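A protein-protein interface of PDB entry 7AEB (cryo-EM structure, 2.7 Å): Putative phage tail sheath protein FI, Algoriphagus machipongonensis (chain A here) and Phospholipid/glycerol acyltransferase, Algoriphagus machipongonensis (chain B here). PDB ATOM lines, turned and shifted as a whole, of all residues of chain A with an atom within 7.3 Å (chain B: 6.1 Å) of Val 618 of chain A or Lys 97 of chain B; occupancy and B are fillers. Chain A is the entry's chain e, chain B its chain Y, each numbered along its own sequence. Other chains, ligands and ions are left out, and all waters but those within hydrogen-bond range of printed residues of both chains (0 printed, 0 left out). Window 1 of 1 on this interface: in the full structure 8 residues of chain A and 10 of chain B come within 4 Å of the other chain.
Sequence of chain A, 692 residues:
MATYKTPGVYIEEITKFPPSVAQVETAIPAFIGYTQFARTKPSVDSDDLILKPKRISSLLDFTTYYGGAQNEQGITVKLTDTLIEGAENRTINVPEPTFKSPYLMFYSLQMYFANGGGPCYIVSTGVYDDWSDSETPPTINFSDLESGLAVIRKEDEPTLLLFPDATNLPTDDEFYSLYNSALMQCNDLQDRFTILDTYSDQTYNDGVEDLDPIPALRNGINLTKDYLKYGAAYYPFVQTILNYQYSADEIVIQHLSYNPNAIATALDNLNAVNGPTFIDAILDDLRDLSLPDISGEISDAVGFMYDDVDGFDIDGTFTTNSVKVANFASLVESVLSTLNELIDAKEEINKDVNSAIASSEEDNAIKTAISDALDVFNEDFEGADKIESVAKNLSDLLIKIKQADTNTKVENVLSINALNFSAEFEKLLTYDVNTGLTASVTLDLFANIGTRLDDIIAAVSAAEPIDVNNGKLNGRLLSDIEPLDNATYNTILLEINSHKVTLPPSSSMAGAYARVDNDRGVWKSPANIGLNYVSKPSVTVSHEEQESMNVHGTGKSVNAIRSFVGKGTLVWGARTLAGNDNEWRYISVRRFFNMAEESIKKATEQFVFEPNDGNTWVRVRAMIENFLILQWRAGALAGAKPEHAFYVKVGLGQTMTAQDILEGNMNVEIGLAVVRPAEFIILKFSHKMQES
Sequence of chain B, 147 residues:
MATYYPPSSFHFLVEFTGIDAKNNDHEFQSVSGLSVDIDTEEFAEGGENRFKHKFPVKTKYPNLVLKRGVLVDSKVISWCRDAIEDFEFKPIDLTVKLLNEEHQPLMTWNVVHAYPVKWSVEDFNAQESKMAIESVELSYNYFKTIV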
ATOM      1  N   PHE A 607     -24.385 -20.753 -23.585  1.00  0.00           N
ATOM      2  CA  PHE A 607     -24.724 -19.724 -24.556  1.00  0.00           C
ATOM      3  C   PHE A 607     -24.691 -20.204 -26.003  1.00  0.00           C
ATOM      4  O   PHE A 607     -24.881 -19.397 -26.911  1.00  0.00           O
ATOM      5  CB  PHE A 607     -23.766 -18.552 -24.446  1.00  0.00           C
ATOM      6  CG  PHE A 607     -23.775 -17.882 -23.138  1.00  0.00           C
ATOM      7  CD1 PHE A 607     -22.771 -18.126 -22.241  1.00  0.00           C
ATOM      8  CD2 PHE A 607     -24.766 -16.998 -22.797  1.00  0.00           C
ATOM      9  CE1 PHE A 607     -22.751 -17.508 -21.036  1.00  0.00           C
ATOM     10  CE2 PHE A 607     -24.745 -16.382 -21.580  1.00  0.00           C
ATOM     11  CZ  PHE A 607     -23.733 -16.640 -20.700  1.00  0.00           C
ATOM     12  N   ASP A 613     -25.841 -11.323 -30.590  1.00  0.00           N
ATOM     13  CA  ASP A 613     -26.071  -9.887 -30.505  1.00  0.00           C
ATOM     14  C   ASP A 613     -25.525  -9.378 -29.159  1.00  0.00           C
ATOM     15  O   ASP A 613     -25.123 -10.165 -28.299  1.00  0.00           O
ATOM     16  CB  ASP A 613     -27.580  -9.624 -30.630  1.00  0.00           C
ATOM     17  CG  ASP A 613     -27.937  -8.211 -31.078  1.00  0.00           C
ATOM     18  OD1 ASP A 613     -27.139  -7.299 -30.919  1.00  0.00           O
ATOM     19  OD2 ASP A 613     -29.034  -8.034 -31.585  1.00  0.00           O
ATOM     20  N   GLY A 614     -25.642  -8.062 -28.948  1.00  0.00           N
ATOM     21  CA  GLY A 614     -25.121  -7.382 -27.765  1.00  0.00           C
ATOM     22  C   GLY A 614     -25.614  -7.908 -26.429  1.00  0.00           C
ATOM     23  O   GLY A 614     -24.866  -7.902 -25.449  1.00  0.00           O
ATOM     24  N   ASN A 615     -26.844  -8.421 -26.380  1.00  0.00           N
ATOM     25  CA  ASN A 615     -27.396  -8.930 -25.131  1.00  0.00           C
ATOM     26  C   ASN A 615     -26.798 -10.259 -24.707  1.00  0.00           C
ATOM     27  O   ASN A 615     -27.018 -10.699 -23.574  1.00  0.00           O
ATOM     28  CB  ASN A 615     -28.897  -9.072 -25.247  1.00  0.00           C
ATOM     29  CG  ASN A 615     -29.596  -7.760 -25.256  1.00  0.00           C
ATOM     30  OD1 ASN A 615     -29.097  -6.755 -24.750  1.00  0.00           O
ATOM     31  ND2 ASN A 615     -30.759  -7.745 -25.838  1.00  0.00           N
ATOM     32  N   THR A 616     -26.052 -10.900 -25.589  1.00  0.00           N
ATOM     33  CA  THR A 616     -25.389 -12.143 -25.284  1.00  0.00           C
ATOM     34  C   THR A 616     -23.933 -11.850 -25.040  1.00  0.00           C
ATOM     35  O   THR A 616     -23.361 -12.323 -24.060  1.00  0.00           O
ATOM     36  CB  THR A 616     -25.542 -13.161 -26.428  1.00  0.00           C
ATOM     37  OG1 THR A 616     -26.933 -13.391 -26.692  1.00  0.00           O
ATOM     38  CG2 THR A 616     -24.887 -14.492 -26.037  1.00  0.00           C
ATOM     39  N   TRP A 617     -23.356 -10.992 -25.872  1.00  0.00           N
ATOM     40  CA  TRP A 617     -21.936 -10.692 -25.775  1.00  0.00           C
ATOM     41  C   TRP A 617     -21.581 -10.197 -24.377  1.00  0.00           C
ATOM     42  O   TRP A 617     -20.607 -10.659 -23.770  1.00  0.00           O
ATOM     43  CB  TRP A 617     -21.571  -9.642 -26.822  1.00  0.00           C
ATOM     44  CG  TRP A 617     -21.877 -10.076 -28.222  1.00  0.00           C
ATOM     45  CD1 TRP A 617     -22.135 -11.329 -28.639  1.00  0.00           C
ATOM     46  CD2 TRP A 617     -21.984  -9.261 -29.381  1.00  0.00           C
ATOM     47  NE1 TRP A 617     -22.398 -11.348 -29.948  1.00  0.00           N
ATOM     48  CE2 TRP A 617     -22.319 -10.092 -30.429  1.00  0.00           C
ATOM     49  CE3 TRP A 617     -21.838  -7.910 -29.624  1.00  0.00           C
ATOM     50  CZ2 TRP A 617     -22.519  -9.639 -31.689  1.00  0.00           C
ATOM     51  CZ3 TRP A 617     -22.037  -7.448 -30.903  1.00  0.00           C
ATOM     52  CH2 TRP A 617     -22.373  -8.304 -31.911  1.00  0.00           C
ATOM     53  N   VAL A 618     -22.437  -9.349 -23.823  1.00  0.00           N
ATOM     54  CA  VAL A 618     -22.249  -8.808 -22.484  1.00  0.00           C
ATOM     55  C   VAL A 618     -22.338  -9.862 -21.376  1.00  0.00           C
ATOM     56  O   VAL A 618     -21.686  -9.719 -20.333  1.00  0.00           O
ATOM     57  CB  VAL A 618     -23.261  -7.675 -22.249  1.00  0.00           C
ATOM     58  CG1 VAL A 618     -24.689  -8.210 -22.102  1.00  0.00           C
ATOM     59  CG2 VAL A 618     -22.856  -6.873 -21.040  1.00  0.00           C
ATOM     60  N   ARG A 619     -23.226 -10.846 -21.527  1.00  0.00           N
ATOM     61  CA  ARG A 619     -23.366 -11.905 -20.550  1.00  0.00           C
ATOM     62  C   ARG A 619     -22.172 -12.840 -20.546  1.00  0.00           C
ATOM     63  O   ARG A 619     -21.771 -13.293 -19.483  1.00  0.00           O
ATOM     64  CB  ARG A 619     -24.680 -12.653 -20.754  1.00  0.00           C
ATOM     65  CG  ARG A 619     -25.874 -11.730 -20.688  1.00  0.00           C
ATOM     66  CD  ARG A 619     -26.952 -12.289 -19.793  1.00  0.00           C
ATOM     67  NE  ARG A 619     -27.655 -13.390 -20.429  1.00  0.00           N
ATOM     68  CZ  ARG A 619     -28.177 -14.423 -19.783  1.00  0.00           C
ATOM     69  NH1 ARG A 619     -28.069 -14.525 -18.467  1.00  0.00           N
ATOM     70  NH2 ARG A 619     -28.788 -15.368 -20.468  1.00  0.00           N
ATOM     71  N   VAL A 620     -21.613 -13.131 -21.722  1.00  0.00           N
ATOM     72  CA  VAL A 620     -20.438 -13.975 -21.853  1.00  0.00           C
ATOM     73  C   VAL A 620     -19.260 -13.306 -21.180  1.00  0.00           C
ATOM     74  O   VAL A 620     -18.533 -13.943 -20.415  1.00  0.00           O
ATOM     75  CB  VAL A 620     -20.161 -14.272 -23.339  1.00  0.00           C
ATOM     76  CG1 VAL A 620     -18.818 -14.967 -23.518  1.00  0.00           C
ATOM     77  CG2 VAL A 620     -21.273 -15.153 -23.873  1.00  0.00           C
ATOM     78  N   ARG A 621     -19.080 -12.006 -21.423  1.00  0.00           N
ATOM     79  CA  ARG A 621     -17.995 -11.297 -20.761  1.00  0.00           C
ATOM     80  C   ARG A 621     -18.104 -11.311 -19.254  1.00  0.00           C
ATOM     81  O   ARG A 621     -17.114 -11.595 -18.580  1.00  0.00           O
ATOM     82  CB  ARG A 621     -17.932  -9.849 -21.162  1.00  0.00           C
ATOM     83  CG  ARG A 621     -17.359  -9.555 -22.487  1.00  0.00           C
ATOM     84  CD  ARG A 621     -17.337  -8.096 -22.708  1.00  0.00           C
ATOM     85  NE  ARG A 621     -16.583  -7.434 -21.640  1.00  0.00           N
ATOM     86  CZ  ARG A 621     -16.499  -6.115 -21.442  1.00  0.00           C
ATOM     87  NH1 ARG A 621     -17.091  -5.267 -22.267  1.00  0.00           N
ATOM     88  NH2 ARG A 621     -15.820  -5.664 -20.397  1.00  0.00           N
ATOM     89  N   ALA A 622     -19.283 -11.017 -18.706  1.00  0.00           N
ATOM     90  CA  ALA A 622     -19.394 -10.949 -17.258  1.00  0.00           C
ATOM     91  C   ALA A 622     -19.014 -12.259 -16.599  1.00  0.00           C
ATOM     92  O   ALA A 622     -18.276 -12.278 -15.612  1.00  0.00           O
ATOM     93  CB  ALA A 622     -20.809 -10.586 -16.874  1.00  0.00           C
ATOM     94  N   MET A 623     -19.448 -13.358 -17.190  1.00  0.00           N
ATOM     95  CA  MET A 623     -19.153 -14.664 -16.644  1.00  0.00           C
ATOM     96  C   MET A 623     -17.670 -15.002 -16.658  1.00  0.00           C
ATOM     97  O   MET A 623     -17.137 -15.517 -15.666  1.00  0.00           O
ATOM     98  CB  MET A 623     -19.915 -15.681 -17.431  1.00  0.00           C
ATOM     99  CG  MET A 623     -19.666 -17.061 -16.987  1.00  0.00           C
ATOM    100  SD  MET A 623     -20.425 -18.174 -18.054  1.00  0.00           S
ATOM    101  CE  MET A 623     -19.323 -18.054 -19.453  1.00  0.00           C
ATOM    102  N   GLU A 625     -15.127 -12.946 -16.735  1.00  0.00           N
ATOM    103  CA  GLU A 625     -14.442 -12.085 -15.785  1.00  0.00           C
ATOM    104  C   GLU A 625     -14.610 -12.585 -14.356  1.00  0.00           C
ATOM    105  O   GLU A 625     -13.650 -12.554 -13.585  1.00  0.00           O
ATOM    106  CB  GLU A 625     -14.951 -10.653 -15.911  1.00  0.00           C
ATOM    107  CG  GLU A 625     -14.541  -9.937 -17.199  1.00  0.00           C
ATOM    108  CD  GLU A 625     -15.210  -8.590 -17.355  1.00  0.00           C
ATOM    109  OE1 GLU A 625     -16.047  -8.267 -16.531  1.00  0.00           O
ATOM    110  OE2 GLU A 625     -14.895  -7.866 -18.295  1.00  0.00           O
ATOM    111  N   VAL A 650     -14.955  -8.664 -26.453  1.00  0.00           N
ATOM    112  CA  VAL A 650     -15.976  -9.246 -27.321  1.00  0.00           C
ATOM    113  C   VAL A 650     -16.730  -8.148 -28.048  1.00  0.00           C
ATOM    114  O   VAL A 650     -17.267  -7.261 -27.390  1.00  0.00           O
ATOM    115  CB  VAL A 650     -17.005 -10.054 -26.508  1.00  0.00           C
ATOM    116  CG1 VAL A 650     -18.025 -10.697 -27.427  1.00  0.00           C
ATOM    117  CG2 VAL A 650     -16.337 -11.084 -25.679  1.00  0.00           C
ATOM    118  N   MET A 666     -18.749 -16.452 -33.152  1.00  0.00           N
ATOM    119  CA  MET A 666     -18.562 -15.468 -32.095  1.00  0.00           C
ATOM    120  C   MET A 666     -17.126 -15.544 -31.608  1.00  0.00           C
ATOM    121  O   MET A 666     -16.659 -16.608 -31.203  1.00  0.00           O
ATOM    122  CB  MET A 666     -19.557 -15.697 -30.961  1.00  0.00           C
ATOM    123  CG  MET A 666     -19.418 -14.735 -29.812  1.00  0.00           C
ATOM    124  SD  MET A 666     -20.675 -14.955 -28.565  1.00  0.00           S
ATOM    125  CE  MET A 666     -20.009 -13.861 -27.354  1.00  0.00           C
ATOM    126  N   HIS B  11     -37.212   1.379 -19.162  1.00  0.00           N
ATOM    127  CA  HIS B  11     -37.022   0.240 -20.060  1.00  0.00           C
ATOM    128  C   HIS B  11     -35.746  -0.513 -19.674  1.00  0.00           C
ATOM    129  O   HIS B  11     -34.631  -0.017 -19.877  1.00  0.00           O
ATOM    130  CB  HIS B  11     -37.041   0.760 -21.506  1.00  0.00           C
ATOM    131  CG  HIS B  11     -37.011  -0.281 -22.576  1.00  0.00           C
ATOM    132  ND1 HIS B  11     -37.926  -1.305 -22.667  1.00  0.00           N
ATOM    133  CD2 HIS B  11     -36.213  -0.394 -23.660  1.00  0.00           C
ATOM    134  CE1 HIS B  11     -37.663  -2.032 -23.735  1.00  0.00           C
ATOM    135  NE2 HIS B  11     -36.629  -1.499 -24.356  1.00  0.00           N
ATOM    136  N   PHE B  12     -35.929  -1.713 -19.103  1.00  0.00           N
ATOM    137  CA  PHE B  12     -34.860  -2.511 -18.503  1.00  0.00           C
ATOM    138  C   PHE B  12     -35.194  -4.010 -18.439  1.00  0.00           C
ATOM    139  O   PHE B  12     -36.355  -4.402 -18.497  1.00  0.00           O
ATOM    140  CB  PHE B  12     -34.561  -1.992 -17.089  1.00  0.00           C
ATOM    141  CG  PHE B  12     -35.768  -1.991 -16.172  1.00  0.00           C
ATOM    142  CD1 PHE B  12     -36.085  -3.090 -15.393  1.00  0.00           C
ATOM    143  CD2 PHE B  12     -36.586  -0.883 -16.090  1.00  0.00           C
ATOM    144  CE1 PHE B  12     -37.210  -3.081 -14.589  1.00  0.00           C
ATOM    145  CE2 PHE B  12     -37.691  -0.877 -15.272  1.00  0.00           C
ATOM    146  CZ  PHE B  12     -37.994  -1.978 -14.515  1.00  0.00           C
ATOM    147  N   LEU B  13     -34.158  -4.835 -18.202  1.00  0.00           N
ATOM    148  CA  LEU B  13     -34.253  -6.302 -18.169  1.00  0.00           C
ATOM    149  C   LEU B  13     -33.482  -6.936 -16.996  1.00  0.00           C
ATOM    150  O   LEU B  13     -32.350  -6.540 -16.747  1.00  0.00           O
ATOM    151  CB  LEU B  13     -33.659  -6.830 -19.469  1.00  0.00           C
ATOM    152  CG  LEU B  13     -33.693  -8.175 -20.052  1.00  0.00           C
ATOM    153  CD1 LEU B  13     -34.928  -8.893 -19.927  1.00  0.00           C
ATOM    154  CD2 LEU B  13     -33.063  -8.212 -21.346  1.00  0.00           C
ATOM    155  N   VAL B  14     -34.032  -7.942 -16.307  1.00  0.00           N
ATOM    156  CA  VAL B  14     -33.317  -8.631 -15.217  1.00  0.00           C
ATOM    157  C   VAL B  14     -33.066 -10.085 -15.616  1.00  0.00           C
ATOM    158  O   VAL B  14     -34.015 -10.817 -15.886  1.00  0.00           O
ATOM    159  CB  VAL B  14     -34.103  -8.570 -13.897  1.00  0.00           C
ATOM    160  CG1 VAL B  14     -33.368  -9.317 -12.787  1.00  0.00           C
ATOM    161  CG2 VAL B  14     -34.356  -7.129 -13.506  1.00  0.00           C
ATOM    162  N   GLU B  15     -31.801 -10.522 -15.642  1.00  0.00           N
ATOM    163  CA  GLU B  15     -31.490 -11.906 -16.002  1.00  0.00           C
ATOM    164  C   GLU B  15     -30.710 -12.620 -14.911  1.00  0.00           C
ATOM    165  O   GLU B  15     -29.876 -12.036 -14.231  1.00  0.00           O
ATOM    166  CB  GLU B  15     -30.684 -12.030 -17.326  1.00  0.00           C
ATOM    167  CG  GLU B  15     -31.399 -11.329 -18.430  1.00  0.00           C
ATOM    168  CD  GLU B  15     -31.653 -12.179 -19.617  1.00  0.00           C
ATOM    169  OE1 GLU B  15     -31.211 -11.907 -20.743  1.00  0.00           O
ATOM    170  OE2 GLU B  15     -32.183 -13.268 -19.327  1.00  0.00           O
ATOM    171  N   THR B  95     -27.680 -10.105 -13.782  1.00  0.00           N
ATOM    172  CA  THR B  95     -27.390  -8.944 -14.616  1.00  0.00           C
ATOM    173  C   THR B  95     -28.563  -7.999 -14.708  1.00  0.00           C
ATOM    174  O   THR B  95     -29.681  -8.422 -14.992  1.00  0.00           O
ATOM    175  CB  THR B  95     -26.885  -9.323 -16.026  1.00  0.00           C
ATOM    176  OG1 THR B  95     -25.797 -10.246 -15.950  1.00  0.00           O
ATOM    177  CG2 THR B  95     -26.534  -8.119 -16.846  1.00  0.00           C
ATOM    178  N   VAL B  96     -28.319  -6.717 -14.457  1.00  0.00           N
ATOM    179  CA  VAL B  96     -29.346  -5.698 -14.616  1.00  0.00           C
ATOM    180  C   VAL B  96     -28.993  -4.883 -15.846  1.00  0.00           C
ATOM    181  O   VAL B  96     -27.890  -4.348 -15.932  1.00  0.00           O
ATOM    182  CB  VAL B  96     -29.458  -4.779 -13.386  1.00  0.00           C
ATOM    183  CG1 VAL B  96     -30.423  -3.636 -13.661  1.00  0.00           C
ATOM    184  CG2 VAL B  96     -29.897  -5.572 -12.164  1.00  0.00           C
ATOM    185  N   LYS B  97     -29.917  -4.768 -16.789  1.00  0.00           N
ATOM    186  CA  LYS B  97     -29.629  -4.061 -18.032  1.00  0.00           C
ATOM    187  C   LYS B  97     -30.534  -2.858 -18.239  1.00  0.00           C
ATOM    188  O   LYS B  97     -31.750  -3.001 -18.240  1.00  0.00           O
ATOM    189  CB  LYS B  97     -29.804  -4.982 -19.233  1.00  0.00           C
ATOM    190  CG  LYS B  97     -28.901  -6.188 -19.269  1.00  0.00           C
ATOM    191  CD  LYS B  97     -29.213  -7.075 -20.460  1.00  0.00           C
ATOM    192  CE  LYS B  97     -28.246  -8.240 -20.552  1.00  0.00           C
ATOM    193  NZ  LYS B  97     -28.600  -9.198 -21.642  1.00  0.00           N
ATOM    194  N   LEU B  98     -29.950  -1.698 -18.498  1.00  0.00           N
ATOM    195  CA  LEU B  98     -30.701  -0.504 -18.871  1.00  0.00           C
ATOM    196  C   LEU B  98     -30.633  -0.404 -20.391  1.00  0.00           C
ATOM    197  O   LEU B  98     -29.537  -0.399 -20.947  1.00  0.00           O
ATOM    198  CB  LEU B  98     -30.109   0.733 -18.188  1.00  0.00           C
ATOM    199  CG  LEU B  98     -30.755   2.093 -18.449  1.00  0.00           C
ATOM    200  CD1 LEU B  98     -32.165   2.149 -17.860  1.00  0.00           C
ATOM    201  CD2 LEU B  98     -29.878   3.179 -17.863  1.00  0.00           C
ATOM    202  N   LEU B  99     -31.782  -0.358 -21.071  1.00  0.00           N
ATOM    203  CA  LEU B  99     -31.820  -0.489 -22.530  1.00  0.00           C
ATOM    204  C   LEU B  99     -32.060   0.789 -23.342  1.00  0.00           C
ATOM    205  O   LEU B  99     -32.736   1.720 -22.902  1.00  0.00           O
ATOM    206  CB  LEU B  99     -32.907  -1.464 -22.931  1.00  0.00           C
ATOM    207  CG  LEU B  99     -32.852  -2.879 -22.390  1.00  0.00           C
ATOM    208  CD1 LEU B  99     -34.076  -3.574 -22.888  1.00  0.00           C
ATOM    209  CD2 LEU B  99     -31.599  -3.593 -22.840  1.00  0.00           C
ATOM    210  N   PRO B 105     -28.342  -2.917 -24.575  1.00  0.00           N
ATOM    211  CA  PRO B 105     -27.887  -2.227 -23.352  1.00  0.00           C
ATOM    212  C   PRO B 105     -27.176  -0.897 -23.566  1.00  0.00           C
ATOM    213  O   PRO B 105     -26.230  -0.803 -24.343  1.00  0.00           O
ATOM    214  CB  PRO B 105     -26.904  -3.230 -22.759  1.00  0.00           C
ATOM    215  CG  PRO B 105     -27.290  -4.542 -23.341  1.00  0.00           C
ATOM    216  CD  PRO B 105     -27.771  -4.264 -24.697  1.00  0.00           C
ATOM    217  N   MET B 107     -26.113   0.435 -20.575  1.00  0.00           N
ATOM    218  CA  MET B 107     -25.255   0.183 -19.434  1.00  0.00           C
ATOM    219  C   MET B 107     -25.748  -1.019 -18.638  1.00  0.00           C
ATOM    220  O   MET B 107     -26.960  -1.215 -18.496  1.00  0.00           O
ATOM    221  CB  MET B 107     -25.228   1.409 -18.536  1.00  0.00           C
ATOM    222  CG  MET B 107     -24.495   1.216 -17.251  1.00  0.00           C
ATOM    223  SD  MET B 107     -24.325   2.709 -16.338  1.00  0.00           S
ATOM    224  CE  MET B 107     -23.293   2.059 -15.056  1.00  0.00           C
ATOM    225  N   THR B 108     -24.811  -1.826 -18.097  1.00  0.00           N
ATOM    226  CA  THR B 108     -25.260  -2.939 -17.282  1.00  0.00           C
ATOM    227  C   THR B 108     -24.540  -2.984 -15.929  1.00  0.00           C
ATOM    228  O   THR B 108     -23.443  -2.447 -15.739  1.00  0.00           O
ATOM    229  CB  THR B 108     -25.004  -4.302 -17.923  1.00  0.00           C
ATOM    230  OG1 THR B 108     -23.613  -4.487 -18.147  1.00  0.00           O
ATOM    231  CG2 THR B 108     -25.615  -4.295 -19.328  1.00  0.00           C
ATOM    232  N   TRP B 109     -25.163  -3.707 -15.001  1.00  0.00           N
ATOM    233  CA  TRP B 109     -24.638  -3.965 -13.669  1.00  0.00           C
ATOM    234  C   TRP B 109     -24.476  -5.463 -13.471  1.00  0.00           C
ATOM    235  O   TRP B 109     -25.412  -6.237 -13.693  1.00  0.00           O
ATOM    236  CB  TRP B 109     -25.564  -3.405 -12.578  1.00  0.00           C
ATOM    237  CG  TRP B 109     -25.644  -1.904 -12.507  1.00  0.00           C
ATOM    238  CD1 TRP B 109     -25.048  -1.111 -11.590  1.00  0.00           C
ATOM    239  CD2 TRP B 109     -26.366  -1.025 -13.385  1.00  0.00           C
ATOM    240  NE1 TRP B 109     -25.334   0.199 -11.840  1.00  0.00           N
ATOM    241  CE2 TRP B 109     -26.140   0.277 -12.941  1.00  0.00           C
ATOM    242  CE3 TRP B 109     -27.174  -1.217 -14.506  1.00  0.00           C
ATOM    243  CZ2 TRP B 109     -26.680   1.370 -13.573  1.00  0.00           C
ATOM    244  CZ3 TRP B 109     -27.705  -0.134 -15.133  1.00  0.00           C
ATOM    245  CH2 TRP B 109     -27.461   1.140 -14.672  1.00  0.00           C
ATOM    246  N   ILE B 146     -20.454  -2.260 -16.443  1.00  0.00           N
ATOM    247  CA  ILE B 146     -19.928  -2.335 -17.794  1.00  0.00           C
ATOM    248  C   ILE B 146     -20.630  -1.314 -18.666  1.00  0.00           C
ATOM    249  O   ILE B 146     -21.861  -1.328 -18.776  1.00  0.00           O
ATOM    250  CB  ILE B 146     -20.097  -3.742 -18.382  1.00  0.00           C
ATOM    251  CG1 ILE B 146     -19.352  -4.761 -17.509  1.00  0.00           C
ATOM    252  CG2 ILE B 146     -19.602  -3.761 -19.822  1.00  0.00           C
ATOM    253  CD1 ILE B 146     -19.633  -6.201 -17.835  1.00  0.00           C
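The backbone carbonyl oxygen (O) of Asn 615 of chain A is in hydrogen-bond range of the side-chain amino group (NZ) of Lys 97 of chain B (2.9 Å).
The guanidinium group (NE) of Arg 619 of chain A is in salt-bridge range of the side-chain carboxylate (OE1) of Glu 15 of chain B, 3.9 Å away.
O of Glu 15 of chain B sits at hydrogen-bond distance from N of Thr 95 of chain B, 3.0 Å away.
O of Leu 13 of chain B is in hydrogen-bond range of N of Lys 97 of chain B, 3.0 Å away.
The backbone NH (N) of Thr 108 of chain B is in hydrogen-bond range of the backbone carbonyl oxygen (O) of Ile 146 of chain B (3.1 Å).
OE1 of Glu 15 of chain B is in salt-bridge range of NZ of Lys 97 of chain B (3.9 Å).
The side-chain carboxylate (OE2) of Glu 625 of chain A is in salt-bridge range of the guanidinium group (NH2) of Arg 621 of chain A, at 3.2 Å.
Among the printed residues, merely in contact across the chains: Asn 615 of chain A with Pro 105 of chain B (2.8 Å), Arg 621 of chain A with Ile 146 of chain B (3.8 Å), Val 618 of chain A with Thr 108 of chain B (3.8 Å), Arg 619 of chain A with Lys 97 of chain B (3.8 Å) and Val 618 of chain A with Lys 97 of chain B (3.9 Å).
Val 618 of chain A touches just these residues of chain B: Lys 97 (3.9 Å) and Thr 108 (3.8 Å).
Printed residues of chain A within 4 Å of Lys 97 of chain B: Asn 615 (2.9 Å), Val 618 (3.9 Å) and Arg 619 (3.8 Å).
Of the printed residues of chain A, Glu 15 of chain B touches Arg 619 (3.8 Å).
Of the printed residues of chain A, Ile 146 of chain B touches Arg 621.
Val 96 of chain B touches none of the printed residues of chain A.
Leu 99 of chain B touches none of the printed residues of chain A.
The nearest residue of chain B that does not touch Val 618 of chain A is Ile 146 of chain B (4.6 Å).
The nearest printed residue of chain A that does not touch Ile 146 of chain B is Glu 625 of chain A (4.3 Å).
Of the 15 printed residues of chain A, 4 touch a printed residue of chain B.
Hydrophobic or aromatic side chains of chain A within 4 Å of the printed part of chain B: Val 618.
Printed residues of chain B that touch a printed residue of chain A: Glu 15, Lys 97, Pro 105, Thr 108 and Ile 146.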
